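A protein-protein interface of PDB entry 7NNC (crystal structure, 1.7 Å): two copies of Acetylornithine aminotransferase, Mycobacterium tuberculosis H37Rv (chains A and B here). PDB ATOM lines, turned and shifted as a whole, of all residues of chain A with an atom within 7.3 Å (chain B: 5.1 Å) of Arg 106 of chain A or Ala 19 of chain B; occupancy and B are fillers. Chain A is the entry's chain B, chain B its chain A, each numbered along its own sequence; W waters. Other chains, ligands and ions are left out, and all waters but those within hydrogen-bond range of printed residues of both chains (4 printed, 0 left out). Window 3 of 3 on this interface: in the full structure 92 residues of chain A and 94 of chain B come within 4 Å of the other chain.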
ATOM      1  N   GLU A  95     -17.691 -12.567 -24.959  1.00  0.00           N
ATOM      2  CA  GLU A  95     -17.169 -13.323 -26.097  1.00  0.00           C
ATOM      3  C   GLU A  95     -16.558 -12.401 -27.149  1.00  0.00           C
ATOM      4  O   GLU A  95     -15.464 -12.670 -27.662  1.00  0.00           O
ATOM      5  CB  GLU A  95     -18.291 -14.165 -26.700  1.00  0.00           C
ATOM      6  CG  GLU A  95     -18.636 -15.359 -25.827  1.00  0.00           C
ATOM      7  CD  GLU A  95     -19.938 -16.035 -26.226  1.00  0.00           C
ATOM      8  OE1 GLU A  95     -20.704 -15.453 -27.035  1.00  0.00           O
ATOM      9  OE2 GLU A  95     -20.194 -17.153 -25.725  1.00  0.00           O
ATOM     10  N   VAL A  98     -13.259 -10.786 -25.889  1.00  0.00           N
ATOM     11  CA  VAL A  98     -12.163 -11.753 -25.886  1.00  0.00           C
ATOM     12  C   VAL A  98     -11.662 -11.983 -27.308  1.00  0.00           C
ATOM     13  O   VAL A  98     -10.452 -12.068 -27.553  1.00  0.00           O
ATOM     14  CB  VAL A  98     -12.620 -13.064 -25.215  1.00  0.00           C
ATOM     15  CG1 VAL A  98     -11.646 -14.186 -25.503  1.00  0.00           C
ATOM     16  CG2 VAL A  98     -12.759 -12.848 -23.701  1.00  0.00           C
ATOM     17  N   ALA A 103      -5.867 -12.924 -27.549  1.00  0.00           N
ATOM     18  CA  ALA A 103      -4.793 -13.582 -26.819  1.00  0.00           C
ATOM     19  C   ALA A 103      -4.741 -15.061 -27.176  1.00  0.00           C
ATOM     20  O   ALA A 103      -5.753 -15.676 -27.514  1.00  0.00           O
ATOM     21  CB  ALA A 103      -4.991 -13.426 -25.310  1.00  0.00           C
ATOM     22  N   ASP A 104      -3.549 -15.647 -27.077  1.00  0.00           N
ATOM     23  CA  ASP A 104      -3.450 -17.072 -27.366  1.00  0.00           C
ATOM     24  C   ASP A 104      -3.776 -17.951 -26.164  1.00  0.00           C
ATOM     25  O   ASP A 104      -3.884 -19.171 -26.327  1.00  0.00           O
ATOM     26  CB  ASP A 104      -2.060 -17.409 -27.930  1.00  0.00           C
ATOM     27  CG  ASP A 104      -0.926 -17.086 -26.968  1.00  0.00           C
ATOM     28  OD1 ASP A 104      -1.051 -17.350 -25.755  1.00  0.00           O
ATOM     29  OD2 ASP A 104       0.107 -16.558 -27.437  1.00  0.00           O
ATOM     30  N   GLN A 105      -3.938 -17.376 -24.975  1.00  0.00           N
ATOM     31  CA  GLN A 105      -4.358 -18.115 -23.794  1.00  0.00           C
ATOM     32  C   GLN A 105      -5.799 -17.772 -23.452  1.00  0.00           C
ATOM     33  O   GLN A 105      -6.347 -16.771 -23.926  1.00  0.00           O
ATOM     34  CB  GLN A 105      -3.456 -17.799 -22.600  1.00  0.00           C
ATOM     35  CG  GLN A 105      -1.988 -17.993 -22.901  1.00  0.00           C
ATOM     36  CD  GLN A 105      -1.116 -17.789 -21.689  1.00  0.00           C
ATOM     37  OE1 GLN A 105      -1.151 -18.572 -20.741  1.00  0.00           O
ATOM     38  NE2 GLN A 105      -0.324 -16.725 -21.709  1.00  0.00           N
ATOM     39  N   ARG A 106      -6.403 -18.606 -22.604  1.00  0.00           N
ATOM     40  CA  ARG A 106      -7.772 -18.354 -22.171  1.00  0.00           C
ATOM     41  C   ARG A 106      -7.877 -16.992 -21.498  1.00  0.00           C
ATOM     42  O   ARG A 106      -7.061 -16.634 -20.640  1.00  0.00           O
ATOM     43  CB  ARG A 106      -8.275 -19.446 -21.227  1.00  0.00           C
ATOM     44  CG  ARG A 106      -9.702 -19.152 -20.739  1.00  0.00           C
ATOM     45  CD  ARG A 106     -10.512 -20.384 -20.382  1.00  0.00           C
ATOM     46  NE  ARG A 106     -10.337 -21.433 -21.378  1.00  0.00           N
ATOM     47  CZ  ARG A 106     -11.275 -21.798 -22.247  1.00  0.00           C
ATOM     48  NH1 ARG A 106     -12.445 -21.170 -22.272  1.00  0.00           N
ATOM     49  NH2 ARG A 106     -11.030 -22.772 -23.116  1.00  0.00           N
ATOM     50  N   THR A 107      -8.873 -16.227 -21.918  1.00  0.00           N
ATOM     51  CA  THR A 107      -9.145 -14.896 -21.398  1.00  0.00           C
ATOM     52  C   THR A 107     -10.526 -14.887 -20.770  1.00  0.00           C
ATOM     53  O   THR A 107     -11.476 -15.431 -21.344  1.00  0.00           O
ATOM     54  CB  THR A 107      -9.074 -13.865 -22.526  1.00  0.00           C
ATOM     55  OG1 THR A 107      -7.791 -13.955 -23.152  1.00  0.00           O
ATOM     56  CG2 THR A 107      -9.282 -12.453 -21.991  1.00  0.00           C
ATOM     57  N   ARG A 108     -10.643 -14.271 -19.591  1.00  0.00           N
ATOM     58  CA  ARG A 108     -11.915 -14.189 -18.890  1.00  0.00           C
ATOM     59  C   ARG A 108     -12.238 -12.736 -18.568  1.00  0.00           C
ATOM     60  O   ARG A 108     -11.352 -11.882 -18.496  1.00  0.00           O
ATOM     61  CB  ARG A 108     -11.910 -15.033 -17.608  1.00  0.00           C
ATOM     62  CG  ARG A 108     -11.705 -16.513 -17.882  1.00  0.00           C
ATOM     63  CD  ARG A 108     -11.948 -17.343 -16.633  1.00  0.00           C
ATOM     64  NE  ARG A 108     -11.817 -18.759 -16.960  1.00  0.00           N
ATOM     65  CZ  ARG A 108     -12.824 -19.495 -17.417  1.00  0.00           C
ATOM     66  NH1 ARG A 108     -14.018 -18.938 -17.590  1.00  0.00           N
ATOM     67  NH2 ARG A 108     -12.633 -20.771 -17.713  1.00  0.00           N
ATOM     68  N   VAL A 109     -13.522 -12.468 -18.354  1.00  0.00           N
ATOM     69  CA  VAL A 109     -14.045 -11.105 -18.326  1.00  0.00           C
ATOM     70  C   VAL A 109     -14.792 -10.856 -17.020  1.00  0.00           C
ATOM     71  O   VAL A 109     -15.564 -11.706 -16.570  1.00  0.00           O
ATOM     72  CB  VAL A 109     -14.991 -10.860 -19.524  1.00  0.00           C
ATOM     73  CG1 VAL A 109     -15.515  -9.430 -19.492  1.00  0.00           C
ATOM     74  CG2 VAL A 109     -14.284 -11.148 -20.853  1.00  0.00           C
ATOM     75  N   ALA A 268      -8.710 -10.575 -18.260  1.00  0.00           N
ATOM     76  CA  ALA A 268      -7.488 -11.159 -17.723  1.00  0.00           C
ATOM     77  C   ALA A 268      -7.124 -12.379 -18.552  1.00  0.00           C
ATOM     78  O   ALA A 268      -8.006 -13.132 -18.973  1.00  0.00           O
ATOM     79  CB  ALA A 268      -7.633 -11.536 -16.230  1.00  0.00           C
ATOM     80  N   VAL A 269      -5.818 -12.572 -18.769  1.00  0.00           N
ATOM     81  CA  VAL A 269      -5.299 -13.554 -19.715  1.00  0.00           C
ATOM     82  C   VAL A 269      -4.474 -14.599 -18.977  1.00  0.00           C
ATOM     83  O   VAL A 269      -3.665 -14.259 -18.106  1.00  0.00           O
ATOM     84  CB  VAL A 269      -4.443 -12.857 -20.792  1.00  0.00           C
ATOM     85  CG1 VAL A 269      -3.857 -13.877 -21.767  1.00  0.00           C
ATOM     86  CG2 VAL A 269      -5.271 -11.787 -21.504  1.00  0.00           C
ATOM     87  N   GLY A 270      -4.663 -15.869 -19.339  1.00  0.00           N
ATOM     88  CA  GLY A 270      -3.841 -16.930 -18.801  1.00  0.00           C
ATOM     89  C   GLY A 270      -4.060 -17.123 -17.313  1.00  0.00           C
ATOM     90  O   GLY A 270      -5.187 -17.039 -16.819  1.00  0.00           O
ATOM     91  N   PRO A 271      -2.989 -17.390 -16.566  1.00  0.00           N
ATOM     92  CA  PRO A 271      -3.158 -17.627 -15.120  1.00  0.00           C
ATOM     93  C   PRO A 271      -3.880 -16.498 -14.398  1.00  0.00           C
ATOM     94  O   PRO A 271      -4.619 -16.762 -13.439  1.00  0.00           O
ATOM     95  CB  PRO A 271      -1.712 -17.788 -14.630  1.00  0.00           C
ATOM     96  CG  PRO A 271      -0.984 -18.328 -15.829  1.00  0.00           C
ATOM     97  CD  PRO A 271      -1.593 -17.597 -16.997  1.00  0.00           C
ATOM     98  N   ALA A 272      -3.710 -15.247 -14.841  1.00  0.00           N
ATOM     99  CA  ALA A 272      -4.409 -14.146 -14.190  1.00  0.00           C
ATOM    100  C   ALA A 272      -5.919 -14.302 -14.288  1.00  0.00           C
ATOM    101  O   ALA A 272      -6.656 -13.759 -13.457  1.00  0.00           O
ATOM    102  CB  ALA A 272      -3.979 -12.810 -14.804  1.00  0.00           C
ATOM    103  N   ALA A 273      -6.402 -15.015 -15.309  1.00  0.00           N
ATOM    104  CA  ALA A 273      -7.840 -15.160 -15.498  1.00  0.00           C
ATOM    105  C   ALA A 273      -8.484 -16.050 -14.443  1.00  0.00           C
ATOM    106  O   ALA A 273      -9.713 -16.037 -14.308  1.00  0.00           O
ATOM    107  CB  ALA A 273      -8.134 -15.729 -16.887  1.00  0.00           C
ATOM    108  N   GLU A 274      -7.689 -16.822 -13.707  1.00  0.00           N
ATOM    109  CA  GLU A 274      -8.199 -17.793 -12.749  1.00  0.00           C
ATOM    110  C   GLU A 274      -8.043 -17.328 -11.309  1.00  0.00           C
ATOM    111  O   GLU A 274      -8.463 -18.045 -10.390  1.00  0.00           O
ATOM    112  CB  GLU A 274      -7.492 -19.142 -12.951  1.00  0.00           C
ATOM    113  CG  GLU A 274      -7.423 -19.560 -14.433  1.00  0.00           C
ATOM    114  CD  GLU A 274      -8.793 -19.883 -15.023  1.00  0.00           C
ATOM    115  OE1 GLU A 274      -9.651 -20.423 -14.290  1.00  0.00           O
ATOM    116  OE2 GLU A 274      -9.030 -19.564 -16.212  1.00  0.00           O
ATOM    117  N   GLN B  15     -22.759 -23.097 -20.174  1.00  0.00           N
ATOM    118  CA  GLN B  15     -21.441 -23.470 -20.729  1.00  0.00           C
ATOM    119  C   GLN B  15     -20.768 -22.222 -21.322  1.00  0.00           C
ATOM    120  O   GLN B  15     -19.581 -22.095 -21.178  1.00  0.00           O
ATOM    121  CB  GLN B  15     -21.563 -24.570 -21.789  1.00  0.00           C
ATOM    122  N   ARG B  16     -21.525 -21.396 -22.035  1.00  0.00           N
ATOM    123  CA  ARG B  16     -20.934 -20.176 -22.580  1.00  0.00           C
ATOM    124  C   ARG B  16     -20.437 -19.272 -21.459  1.00  0.00           C
ATOM    125  O   ARG B  16     -19.343 -18.708 -21.551  1.00  0.00           O
ATOM    126  CB  ARG B  16     -21.934 -19.431 -23.461  1.00  0.00           C
ATOM    127  CG  ARG B  16     -22.238 -20.089 -24.812  1.00  0.00           C
ATOM    128  CD  ARG B  16     -23.451 -19.400 -25.425  1.00  0.00           C
ATOM    129  NE  ARG B  16     -23.132 -18.013 -25.754  1.00  0.00           N
ATOM    130  CZ  ARG B  16     -24.018 -17.103 -26.153  1.00  0.00           C
ATOM    131  NH1 ARG B  16     -25.304 -17.414 -26.239  1.00  0.00           N
ATOM    132  NH2 ARG B  16     -23.620 -15.866 -26.432  1.00  0.00           N
ATOM    133  N   TRP B  17     -21.210 -19.151 -20.375  1.00  0.00           N
ATOM    134  CA  TRP B  17     -20.745 -18.385 -19.220  1.00  0.00           C
ATOM    135  C   TRP B  17     -19.418 -18.930 -18.695  1.00  0.00           C
ATOM    136  O   TRP B  17     -18.471 -18.174 -18.446  1.00  0.00           O
ATOM    137  CB  TRP B  17     -21.824 -18.393 -18.130  1.00  0.00           C
ATOM    138  CG  TRP B  17     -21.391 -17.793 -16.817  1.00  0.00           C
ATOM    139  CD1 TRP B  17     -20.511 -18.324 -15.913  1.00  0.00           C
ATOM    140  CD2 TRP B  17     -21.772 -16.516 -16.304  1.00  0.00           C
ATOM    141  NE1 TRP B  17     -20.344 -17.462 -14.856  1.00  0.00           N
ATOM    142  CE2 TRP B  17     -21.116 -16.350 -15.065  1.00  0.00           C
ATOM    143  CE3 TRP B  17     -22.625 -15.507 -16.755  1.00  0.00           C
ATOM    144  CZ2 TRP B  17     -21.274 -15.208 -14.281  1.00  0.00           C
ATOM    145  CZ3 TRP B  17     -22.785 -14.367 -15.968  1.00  0.00           C
ATOM    146  CH2 TRP B  17     -22.113 -14.230 -14.747  1.00  0.00           C
ATOM    147  N   GLN B  18     -19.323 -20.250 -18.537  1.00  0.00           N
ATOM    148  CA  GLN B  18     -18.120 -20.829 -17.954  1.00  0.00           C
ATOM    149  C   GLN B  18     -16.911 -20.722 -18.869  1.00  0.00           C
ATOM    150  O   GLN B  18     -15.780 -20.842 -18.390  1.00  0.00           O
ATOM    151  CB  GLN B  18     -18.362 -22.293 -17.586  1.00  0.00           C
ATOM    152  CG  GLN B  18     -19.421 -22.455 -16.510  1.00  0.00           C
ATOM    153  CD  GLN B  18     -19.674 -23.906 -16.132  1.00  0.00           C
ATOM    154  OE1 GLN B  18     -19.753 -24.238 -14.952  1.00  0.00           O
ATOM    155  NE2 GLN B  18     -19.841 -24.769 -17.133  1.00  0.00           N
ATOM    156  N   ALA B  19     -17.116 -20.508 -20.163  1.00  0.00           N
ATOM    157  CA  ALA B  19     -15.988 -20.407 -21.080  1.00  0.00           C
ATOM    158  C   ALA B  19     -15.380 -19.013 -21.118  1.00  0.00           C
ATOM    159  O   ALA B  19     -14.233 -18.869 -21.553  1.00  0.00           O
ATOM    160  CB  ALA B  19     -16.416 -20.803 -22.492  1.00  0.00           C
ATOM    161  N   VAL B  20     -16.103 -17.988 -20.672  1.00  0.00           N
ATOM    162  CA  VAL B  20     -15.638 -16.622 -20.894  1.00  0.00           C
ATOM    163  C   VAL B  20     -15.710 -15.745 -19.650  1.00  0.00           C
ATOM    164  O   VAL B  20     -14.970 -14.748 -19.557  1.00  0.00           O
ATOM    165  CB  VAL B  20     -16.437 -15.968 -22.043  1.00  0.00           C
ATOM    166  CG1 VAL B  20     -17.904 -15.739 -21.641  1.00  0.00           C
ATOM    167  CG2 VAL B  20     -15.748 -14.722 -22.551  1.00  0.00           C
ATOM    168  N   MET B  21     -16.545 -16.027 -18.655  1.00  0.00           N
ATOM    169  CA  MET B  21     -16.649 -15.098 -17.540  1.00  0.00           C
ATOM    170  C   MET B  21     -15.621 -15.449 -16.473  1.00  0.00           C
ATOM    171  O   MET B  21     -15.297 -16.622 -16.269  1.00  0.00           O
ATOM    172  CB  MET B  21     -18.053 -15.114 -16.925  1.00  0.00           C
ATOM    173  CG  MET B  21     -19.084 -14.860 -18.009  1.00  0.00           C
ATOM    174  SD  MET B  21     -19.016 -13.191 -18.685  1.00  0.00           S
ATOM    175  CE  MET B  21     -18.880 -12.166 -17.200  1.00  0.00           C
HETATM  176  O   HOH W   1     -18.571 -18.528 -24.230  1.00  0.00           O
HETATM  177  O   HOH W   2     -14.514 -23.332 -17.182  1.00  0.00           O
HETATM  178  O   HOH W   3     -12.691 -17.052 -23.115  1.00  0.00           O
HETATM  179  O   HOH W   4     -16.492 -18.999 -15.323  1.00  0.00           O
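The guanidinium group of Arg 16 of chain B is in salt-bridge range of the side-chain carboxylate of Glu 95 of chain A, at 3.0 Å. NH1 of Arg 108 of chain A sits at hydrogen-bond distance from O of Gln 18 of chain B, at 2.7 Å. O of Ala 19 of chain B lies within hydrogen-bond range of NH1 of Arg 106 of chain A. The backbone NH (N) of Val 109 of chain A lies within hydrogen-bond range of the backbone carbonyl oxygen (O) of Val 20 of chain B (3.0 Å). The backbone carbonyl oxygen of Met 21 of chain B sits at hydrogen-bond distance from the guanidinium group of Arg 108 of chain A, at 3.0 Å.
The backbone carbonyl oxygen (O) of Gln 105 of chain A is in hydrogen-bond range of the side-chain hydroxyl (OG1) of Thr 107 of chain A (3.3 Å). O of Arg 106 of chain A is in hydrogen-bond range of N of Gly 270 of chain A, 2.8 Å away. The backbone carbonyl oxygen (O) of Ala 268 of chain A lies within hydrogen-bond range of the backbone NH (N) of Arg 108 of chain A, at 2.9 Å. NE of Arg 108 of chain A lies within salt-bridge range of OE2 of Glu 274 of chain A, at 3.0 Å.
Among the printed residues, pairs that only touch across the chains: Glu 95 of chain A with Val 20 of chain B, Val 98 of chain A with Val 20 of chain B, Thr 107 of chain A with Val 20 of chain B, Arg 108 of chain A with Ala 19 of chain B, Arg 108 of chain A with Val 20 of chain B and Val 109 of chain A with Met 21 of chain B.
Arg 106 of chain A touches just one residue of chain B: Ala 19. Of the printed residues of chain B, Thr 107 of chain A touches Val 20. Pro 271 of chain A touches none of the printed residues of chain B. Glu 274 of chain A touches none of the printed residues of chain B. Ala 19 of chain B touches just these residues of chain A: Arg 106 (3.0 Å) and Arg 108 (3.8 Å). Of the printed residues of chain A, Val 20 of chain B touches Glu 95, Val 98, Thr 107, Arg 108 and Val 109. The nearest printed residue of chain B that does not touch Arg 106 of chain A is Val 20 of chain B (5.1 Å). The nearest residue of chain A that does not touch Ala 19 of chain B is Thr 107 of chain A (4.4 Å). The nearest printed residue of chain A that does not touch Gln 18 of chain B is Arg 106 of chain A (5.1 Å).
Of the 16 printed residues of chain A, 6 touch a printed residue of chain B. Printed residues of chain A that touch a printed residue of chain B: Glu 95, Val 98, Arg 106, Thr 107, Arg 108 and Val 109. Hydrophobic or aromatic side chains of chain A that line the printed part of chain B: Val 98 and Val 109. Among the printed residues, 11 pairs touch across the chains.
No position is printed for both chains. Of the 11 pairs that touch across the chains among the printed residues, none has its exchanged pair printed and touching as well.
Water W1 bridges OE2 of Glu 95 of chain A (2.6 Å) and O of Arg 16 of chain B (2.8 Å). Water W3 lies within hydrogen-bond range of O of Thr 107 of chain A (2.7 Å) and O of Ala 19 of chain B (2.8 Å). Water W4 bridges O of Met 21 of chain B and NH1 of Arg 108 of chain A. Water W2 lies within hydrogen-bond range of the backbone carbonyl oxygen (O) of Gln 18 of chain B (3.0 Å) and the guanidinium group (NH2) of Arg 108 of chain A (3.2 Å).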
